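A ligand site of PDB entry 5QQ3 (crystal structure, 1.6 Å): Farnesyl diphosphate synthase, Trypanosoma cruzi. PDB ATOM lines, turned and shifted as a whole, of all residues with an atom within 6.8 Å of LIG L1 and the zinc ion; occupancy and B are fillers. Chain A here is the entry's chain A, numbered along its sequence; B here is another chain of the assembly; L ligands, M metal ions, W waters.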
ATOM      1  N   CYS A 156     -33.440  21.095 -12.534  1.00  0.00           N
ATOM      2  CA  CYS A 156     -34.042  20.457 -11.349  1.00  0.00           C
ATOM      3  C   CYS A 156     -32.906  19.697 -10.591  1.00  0.00           C
ATOM      4  O   CYS A 156     -32.797  19.814  -9.387  1.00  0.00           O
ATOM      5  CB  CYS A 156     -35.134  19.488 -11.800  1.00  0.00           C
ATOM      6  SG  CYS A 156     -35.904  18.785 -10.306  1.00  0.00           S
ATOM      7  N   LEU A 157     -32.069  18.982 -11.325  1.00  0.00           N
ATOM      8  CA  LEU A 157     -30.908  18.266 -10.724  1.00  0.00           C
ATOM      9  C   LEU A 157     -29.901  19.236 -10.060  1.00  0.00           C
ATOM     10  O   LEU A 157     -29.458  19.017  -8.929  1.00  0.00           O
ATOM     11  CB  LEU A 157     -30.203  17.404 -11.711  1.00  0.00           C
ATOM     12  CG  LEU A 157     -29.038  16.572 -11.102  1.00  0.00           C
ATOM     13  CD1 LEU A 157     -29.516  15.645 -10.012  1.00  0.00           C
ATOM     14  CD2 LEU A 157     -28.314  15.874 -12.202  1.00  0.00           C
ATOM     15  N   GLN A 159     -30.369  22.113  -8.946  1.00  0.00           N
ATOM     16  CA  GLN A 159     -31.002  22.705  -7.810  1.00  0.00           C
ATOM     17  C   GLN A 159     -30.962  21.769  -6.564  1.00  0.00           C
ATOM     18  O   GLN A 159     -30.710  22.192  -5.430  1.00  0.00           O
ATOM     19  CB  GLN A 159     -32.419  22.970  -8.331  1.00  0.00           C
ATOM     20  CG  GLN A 159     -33.473  23.497  -7.463  1.00  0.00           C
ATOM     21  CD  GLN A 159     -34.115  22.458  -6.592  1.00  0.00           C
ATOM     22  OE1 GLN A 159     -34.031  22.604  -5.375  1.00  0.00           O
ATOM     23  NE2 GLN A 159     -34.791  21.400  -7.190  1.00  0.00           N
ATOM     24  N   LYS A 160     -31.169  20.487  -6.788  1.00  0.00           N
ATOM     25  CA  LYS A 160     -31.086  19.485  -5.716  1.00  0.00           C
ATOM     26  C   LYS A 160     -29.625  19.260  -5.246  1.00  0.00           C
ATOM     27  O   LYS A 160     -29.381  19.151  -4.012  1.00  0.00           O
ATOM     28  CB  LYS A 160     -31.703  18.163  -6.176  1.00  0.00           C
ATOM     29  CG  LYS A 160     -33.231  18.319  -6.295  1.00  0.00           C
ATOM     30  CD  LYS A 160     -33.795  17.174  -7.057  1.00  0.00           C
ATOM     31  CE  LYS A 160     -35.344  17.211  -7.197  1.00  0.00           C
ATOM     32  NZ  LYS A 160     -35.677  16.222  -8.274  1.00  0.00           N
ATOM     33  N   VAL A 161     -28.672  19.282  -6.174  1.00  0.00           N
ATOM     34  CA  VAL A 161     -27.283  19.151  -5.824  1.00  0.00           C
ATOM     35  C   VAL A 161     -26.829  20.351  -5.036  1.00  0.00           C
ATOM     36  O   VAL A 161     -26.104  20.191  -4.054  1.00  0.00           O
ATOM     37  CB  VAL A 161     -26.350  18.906  -7.030  1.00  0.00           C
ATOM     38  CG1 VAL A 161     -24.853  19.049  -6.691  1.00  0.00           C
ATOM     39  CG2 VAL A 161     -26.629  17.534  -7.619  1.00  0.00           C
ATOM     40  N   ASP A 162     -27.239  21.529  -5.449  1.00  0.00           N
ATOM     41  CA  ASP A 162     -26.844  22.765  -4.667  1.00  0.00           C
ATOM     42  C   ASP A 162     -27.384  22.690  -3.257  1.00  0.00           C
ATOM     43  O   ASP A 162     -26.622  22.929  -2.311  1.00  0.00           O
ATOM     44  CB  ASP A 162     -27.471  23.988  -5.411  1.00  0.00           C
ATOM     45  CG  ASP A 162     -27.264  25.298  -4.717  1.00  0.00           C
ATOM     46  OD1 ASP A 162     -26.236  25.461  -4.096  1.00  0.00           O
ATOM     47  OD2 ASP A 162     -28.024  26.240  -5.040  1.00  0.00           O
ATOM     48  N   ALA A 164     -28.334  19.973  -1.523  1.00  0.00           N
ATOM     49  CA  ALA A 164     -27.536  18.946  -0.814  1.00  0.00           C
ATOM     50  C   ALA A 164     -26.169  19.457  -0.332  1.00  0.00           C
ATOM     51  O   ALA A 164     -25.736  19.107   0.771  1.00  0.00           O
ATOM     52  CB  ALA A 164     -27.338  17.776  -1.742  1.00  0.00           C
ATOM     53  N   LYS A 207     -20.630  12.868   1.831  1.00  0.00           N
ATOM     54  CA  LYS A 207     -21.531  12.666   0.740  1.00  0.00           C
ATOM     55  C   LYS A 207     -22.196  13.968   0.314  1.00  0.00           C
ATOM     56  O   LYS A 207     -22.333  14.243  -0.894  1.00  0.00           O
ATOM     57  CB  LYS A 207     -22.522  11.603   1.107  1.00  0.00           C
ATOM     58  CG  LYS A 207     -23.661  11.394   0.121  1.00  0.00           C
ATOM     59  CD  LYS A 207     -24.468  10.220   0.633  1.00  0.00           C
ATOM     60  CE  LYS A 207     -25.888  10.385   0.487  1.00  0.00           C
ATOM     61  NZ  LYS A 207     -26.584   9.152   0.751  1.00  0.00           N
ATOM     62  N   TYR A 208     -22.714  14.689   1.317  1.00  0.00           N
ATOM     63  CA  TYR A 208     -23.446  15.954   1.104  1.00  0.00           C
ATOM     64  C   TYR A 208     -22.540  17.080   0.735  1.00  0.00           C
ATOM     65  O   TYR A 208     -22.854  17.825  -0.242  1.00  0.00           O
ATOM     66  CB  TYR A 208     -24.414  16.270   2.258  1.00  0.00           C
ATOM     67  CG  TYR A 208     -25.492  15.231   2.191  1.00  0.00           C
ATOM     68  CD1 TYR A 208     -25.385  13.995   2.809  1.00  0.00           C
ATOM     69  CD2 TYR A 208     -26.665  15.495   1.535  1.00  0.00           C
ATOM     70  CE1 TYR A 208     -26.412  13.054   2.733  1.00  0.00           C
ATOM     71  CE2 TYR A 208     -27.661  14.539   1.386  1.00  0.00           C
ATOM     72  CZ  TYR A 208     -27.548  13.311   1.990  1.00  0.00           C
ATOM     73  OH  TYR A 208     -28.540  12.426   1.827  1.00  0.00           O
ATOM     74  N   PHE A 212     -21.890  15.068  -4.160  1.00  0.00           N
ATOM     75  CA  PHE A 212     -23.001  15.385  -5.044  1.00  0.00           C
ATOM     76  C   PHE A 212     -22.480  16.380  -6.057  1.00  0.00           C
ATOM     77  O   PHE A 212     -22.713  16.155  -7.261  1.00  0.00           O
ATOM     78  CB  PHE A 212     -24.255  15.849  -4.312  1.00  0.00           C
ATOM     79  CG  PHE A 212     -25.007  14.755  -3.696  1.00  0.00           C
ATOM     80  CD1 PHE A 212     -25.637  13.798  -4.494  1.00  0.00           C
ATOM     81  CD2 PHE A 212     -25.160  14.683  -2.322  1.00  0.00           C
ATOM     82  CE1 PHE A 212     -26.374  12.765  -3.900  1.00  0.00           C
ATOM     83  CE2 PHE A 212     -25.927  13.719  -1.760  1.00  0.00           C
ATOM     84  CZ  PHE A 212     -26.546  12.732  -2.527  1.00  0.00           C
ATOM     85  N   LEU A 216     -21.329  13.374  -8.697  1.00  0.00           N
ATOM     86  CA  LEU A 216     -22.574  13.058  -9.314  1.00  0.00           C
ATOM     87  C   LEU A 216     -22.938  14.059 -10.395  1.00  0.00           C
ATOM     88  O   LEU A 216     -23.274  13.725 -11.550  1.00  0.00           O
ATOM     89  CB  LEU A 216     -23.649  12.877  -8.273  1.00  0.00           C
ATOM     90  CG  LEU A 216     -25.025  12.548  -8.828  1.00  0.00           C
ATOM     91  CD1 LEU A 216     -24.952  11.169  -9.488  1.00  0.00           C
ATOM     92  CD2 LEU A 216     -26.176  12.635  -7.903  1.00  0.00           C
ATOM     93  N   MET A 234     -29.271   4.930 -13.038  1.00  0.00           N
ATOM     94  CA  MET A 234     -28.937   6.086 -12.221  1.00  0.00           C
ATOM     95  C   MET A 234     -28.570   5.649 -10.793  1.00  0.00           C
ATOM     96  O   MET A 234     -27.627   6.241 -10.214  1.00  0.00           O
ATOM     97  CB  MET A 234     -30.027   7.162 -12.221  1.00  0.00           C
ATOM     98  CG  MET A 234     -29.470   8.514 -11.722  1.00  0.00           C
ATOM     99  SD  MET A 234     -28.055   9.065 -12.760  1.00  0.00           S
ATOM    100  CE  MET A 234     -28.942   9.411 -14.181  1.00  0.00           C
ATOM    101  N   ASN A 235     -29.196   4.572 -10.261  1.00  0.00           N
ATOM    102  CA  ASN A 235     -28.798   4.136  -8.890  1.00  0.00           C
ATOM    103  C   ASN A 235     -27.322   3.706  -8.840  1.00  0.00           C
ATOM    104  O   ASN A 235     -26.576   3.982  -7.831  1.00  0.00           O
ATOM    105  CB  ASN A 235     -29.677   3.025  -8.359  1.00  0.00           C
ATOM    106  CG  ASN A 235     -31.024   3.467  -7.928  1.00  0.00           C
ATOM    107  OD1 ASN A 235     -31.231   4.611  -7.523  1.00  0.00           O
ATOM    108  ND2 ASN A 235     -31.972   2.541  -7.954  1.00  0.00           N
ATOM    109  N   GLU A 238     -25.079   6.915  -8.958  1.00  0.00           N
ATOM    110  CA  GLU A 238     -25.037   7.446  -7.550  1.00  0.00           C
ATOM    111  C   GLU A 238     -24.074   6.686  -6.612  1.00  0.00           C
ATOM    112  O   GLU A 238     -23.204   7.300  -5.905  1.00  0.00           O
ATOM    113  CB  GLU A 238     -26.424   7.597  -6.982  1.00  0.00           C
ATOM    114  CG  GLU A 238     -27.183   8.671  -7.711  1.00  0.00           C
ATOM    115  CD  GLU A 238     -28.448   9.134  -7.042  1.00  0.00           C
ATOM    116  OE1 GLU A 238     -28.718   8.782  -5.877  1.00  0.00           O
ATOM    117  OE2 GLU A 238     -29.271   9.794  -7.727  1.00  0.00           O
ATOM    118  N   HIS A 242     -20.700   8.140  -4.978  1.00  0.00           N
ATOM    119  CA  HIS A 242     -20.512   8.186  -3.482  1.00  0.00           C
ATOM    120  C   HIS A 242     -19.172   7.570  -3.086  1.00  0.00           C
ATOM    121  O   HIS A 242     -18.444   8.094  -2.235  1.00  0.00           O
ATOM    122  CB  HIS A 242     -21.691   7.577  -2.686  1.00  0.00           C
ATOM    123  CG  HIS A 242     -22.986   8.254  -2.992  1.00  0.00           C
ATOM    124  ND1 HIS A 242     -23.077   9.598  -3.351  1.00  0.00           N
ATOM    125  CD2 HIS A 242     -24.257   7.777  -3.039  1.00  0.00           C
ATOM    126  CE1 HIS A 242     -24.331   9.908  -3.620  1.00  0.00           C
ATOM    127  NE2 HIS A 242     -25.065   8.818  -3.454  1.00  0.00           N
ATOM    128  N   GLN B  25     -35.518  14.904   6.293  1.00  0.00           N
ATOM    129  CA  GLN B  25     -35.504  13.596   7.000  1.00  0.00           C
ATOM    130  C   GLN B  25     -35.629  12.403   6.097  1.00  0.00           C
ATOM    131  O   GLN B  25     -34.855  11.428   6.237  1.00  0.00           O
ATOM    132  CB  GLN B  25     -36.629  13.613   7.989  1.00  0.00           C
ATOM    133  CG  GLN B  25     -36.566  12.420   8.916  1.00  0.00           C
ATOM    134  CD  GLN B  25     -37.860  11.687   8.971  1.00  0.00           C
ATOM    135  OE1 GLN B  25     -38.108  10.830   8.104  1.00  0.00           O
ATOM    136  NE2 GLN B  25     -38.710  12.013   9.990  1.00  0.00           N
ATOM    137  N   SER B  26     -36.470  12.449   5.094  1.00  0.00           N
ATOM    138  CA  SER B  26     -36.722  11.244   4.327  1.00  0.00           C
ATOM    139  C   SER B  26     -35.802  11.148   3.155  1.00  0.00           C
ATOM    140  O   SER B  26     -35.537  10.055   2.725  1.00  0.00           O
ATOM    141  CB  SER B  26     -38.182  11.153   3.912  1.00  0.00           C
ATOM    142  OG  SER B  26     -38.474  12.196   3.042  1.00  0.00           O
ATOM    143  N   LYS B  27     -35.193  12.247   2.671  1.00  0.00           N
ATOM    144  CA  LYS B  27     -34.417  12.207   1.455  1.00  0.00           C
ATOM    145  C   LYS B  27     -32.977  12.742   1.579  1.00  0.00           C
ATOM    146  O   LYS B  27     -32.143  12.536   0.712  1.00  0.00           O
ATOM    147  CB  LYS B  27     -35.151  13.034   0.371  1.00  0.00           C
ATOM    148  CG  LYS B  27     -36.586  12.581  -0.081  1.00  0.00           C
ATOM    149  CD  LYS B  27     -36.602  12.773  -1.615  1.00  0.00           C
ATOM    150  CE  LYS B  27     -37.980  12.639  -2.301  1.00  0.00           C
ATOM    151  NZ  LYS B  27     -38.880  11.795  -1.488  1.00  0.00           N
ATOM    152  N   TYR B  28     -32.690  13.487   2.640  1.00  0.00           N
ATOM    153  CA  TYR B  28     -31.344  14.106   2.800  1.00  0.00           C
ATOM    154  C   TYR B  28     -30.695  13.721   4.124  1.00  0.00           C
ATOM    155  O   TYR B  28     -29.692  14.358   4.520  1.00  0.00           O
ATOM    156  CB  TYR B  28     -31.411  15.670   2.639  1.00  0.00           C
ATOM    157  CG  TYR B  28     -31.862  16.169   1.273  1.00  0.00           C
ATOM    158  CD1 TYR B  28     -30.948  16.580   0.342  1.00  0.00           C
ATOM    159  CD2 TYR B  28     -33.183  16.236   0.937  1.00  0.00           C
ATOM    160  CE1 TYR B  28     -31.345  17.036  -0.898  1.00  0.00           C
ATOM    161  CE2 TYR B  28     -33.598  16.679  -0.296  1.00  0.00           C
ATOM    162  CZ  TYR B  28     -32.648  17.067  -1.224  1.00  0.00           C
ATOM    163  OH  TYR B  28     -32.960  17.537  -2.490  1.00  0.00           O
ATOM    164  N   GLU B  29     -31.231  12.676   4.783  1.00  0.00           N
ATOM    165  CA  GLU B  29     -30.606  12.016   5.907  1.00  0.00           C
ATOM    166  C   GLU B  29     -30.423  12.917   7.139  1.00  0.00           C
ATOM    167  O   GLU B  29     -29.488  12.696   7.957  1.00  0.00           O
ATOM    168  CB  GLU B  29     -29.267  11.426   5.496  1.00  0.00           C
ATOM    169  CG  GLU B  29     -29.407  10.300   4.475  1.00  0.00           C
ATOM    170  CD  GLU B  29     -28.062   9.840   3.955  1.00  0.00           C
ATOM    171  OE1 GLU B  29     -27.303   9.227   4.738  1.00  0.00           O
ATOM    172  OE2 GLU B  29     -27.772  10.031   2.779  1.00  0.00           O
HETATM  173  N1  LIG L   1     -30.397  11.666  -5.240  1.00  0.00           N
HETATM  174  C1  LIG L   1     -30.387  11.309  -3.915  1.00  0.00           C
HETATM  175  C2  LIG L   1     -29.951  13.005  -5.341  1.00  0.00           C
HETATM  176  C3  LIG L   1     -29.767  13.857  -6.425  1.00  0.00           C
HETATM  177  C4  LIG L   1     -29.393  15.112  -6.115  1.00  0.00           C
HETATM  178  C5  LIG L   1     -29.242  15.519  -4.815  1.00  0.00           C
HETATM  179  C6  LIG L   1     -29.730  13.377  -4.037  1.00  0.00           C
HETATM  180  N2  LIG L   1     -30.953   9.778  -2.062  1.00  0.00           N
HETATM  181  C7  LIG L   1     -32.113   9.141   1.575  1.00  0.00           C
HETATM  182  O1  LIG L   1     -31.574   9.201   0.255  1.00  0.00           O
HETATM  183  C8  LIG L   1     -30.209   9.380   0.203  1.00  0.00           C
HETATM  184  C9  LIG L   1     -29.881   9.552  -1.236  1.00  0.00           C
HETATM  185  C10 LIG L   1     -30.817   9.938  -3.485  1.00  0.00           C
HETATM  186  C11 LIG L   1     -29.385  14.704  -3.749  1.00  0.00           C
HETATM  187  N3  LIG L   1     -29.976  12.297  -3.145  1.00  0.00           N
HETATM  188  O2  LIG L   1     -28.700   9.530  -1.602  1.00  0.00           O
HETATM  189  N1  LG2 L   2     -33.351  12.259  -9.613  1.00  0.00           N
HETATM  190  C1  LG2 L   2     -33.002  11.688  -8.424  1.00  0.00           C
HETATM  191  C2  LG2 L   2     -32.192  12.276 -10.383  1.00  0.00           C
HETATM  192  C3  LG2 L   2     -31.988  12.675 -11.685  1.00  0.00           C
HETATM  193  C4  LG2 L   2     -30.695  12.491 -12.178  1.00  0.00           C
HETATM  194  C5  LG2 L   2     -29.660  11.965 -11.382  1.00  0.00           C
HETATM  195  C6  LG2 L   2     -31.152  11.734  -9.573  1.00  0.00           C
HETATM  196  N2  LG2 L   2     -33.566  12.074  -6.149  1.00  0.00           N
HETATM  197  C7  LG2 L   2     -33.012  13.883  -2.517  1.00  0.00           C
HETATM  198  O1  LG2 L   2     -33.255  13.267  -3.755  1.00  0.00           O
HETATM  199  C8  LG2 L   2     -33.170  14.164  -4.821  1.00  0.00           C
HETATM  200  C9  LG2 L   2     -33.615  13.424  -6.110  1.00  0.00           C
HETATM  201  C10 LG2 L   2     -34.018  11.390  -7.360  1.00  0.00           C
HETATM  202  C11 LG2 L   2     -29.851  11.600 -10.084  1.00  0.00           C
HETATM  203  N3  LG2 L   2     -31.686  11.367  -8.339  1.00  0.00           N
HETATM  204  O2  LG2 L   2     -33.970  14.073  -7.081  1.00  0.00           O
HETATM  205 ZN    ZN M   1     -30.921  10.397  -6.912  1.00  0.00          ZN
HETATM  206  O   HOH W   1     -33.401  10.243  -1.776  1.00  0.00           O
HETATM  207  O   HOH W   2     -32.102   8.647  -6.475  1.00  0.00           O
HETATM  208  O   HOH W   3     -33.014  10.332   4.249  1.00  0.00           O
HETATM  209  O   HOH W   4     -30.001  12.724  -0.606  1.00  0.00           O
HETATM  210  O   HOH W   5     -27.390   9.550  -3.828  1.00  0.00           O
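An oxygen (O2) of LG2 L2 sits at hydrogen-bond distance from the side-chain amino group of Lys 160.
The side-chain amino group (NZ) of Lys 207 lies within hydrogen-bond range of an oxygen (O2) of LIG L1 (3.2 Å).
The nearest printed residue that does not touch the zinc ion is Leu 216 (5.3 Å).
Water W4 lies within hydrogen-bond range of O of Lys 27 of chain B (2.5 Å), N3 of LIG L1 (2.6 Å) and OH of Tyr 208 (2.9 Å).
Water W5 lies within hydrogen-bond range of a ring nitrogen (NE2) of His 242 (2.5 Å), the side-chain carboxylate of Glu 238 (2.6 Å) and an oxygen (O2) of LIG L1 (2.6 Å).
OE2 of Glu 29 of chain B sits at hydrogen-bond distance from OH of Tyr 208 (2.7 Å).
A ring nitrogen (NE2) of His 242 sits close to the backbone carbonyl oxygen (O) of Glu 238 (3.4 Å).
NZ of Lys 207 lies within salt-bridge range of OE2 of Glu 29 of chain B (2.5 Å).
The side-chain sulfur (SG) of Cys 156 sits at hydrogen-bond distance from the side-chain amino group (NZ) of Lys 160, 3.3 Å away.
The backbone carbonyl oxygen of Lys 207 sits close to the backbone NH of Phe 212 (3.4 Å).
The backbone carbonyl oxygen (O) of Lys 27 of chain B sits close to an oxygen (O1) of LIG L1 (3.4 Å).
Residues that only touch LIG L1: Phe 212, Glu 29 of chain B, Lys 160, Ser 26 of chain B, Tyr 208, Leu 157 and Val 161.
Hydrophobic or aromatic side chains that line LIG L1: Leu 157, Val 161 and Phe 212.
Along chain A the residues within 4 Å of LIG L1 span positions 157 to 238.
The zinc ion is bound by a nitrogen (N3) of LG2 L2, the side-chain carboxylate of Glu 238, water W2 and a nitrogen (N1) of LIG L1.
The zinc ion has four donor atoms within binding distance.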
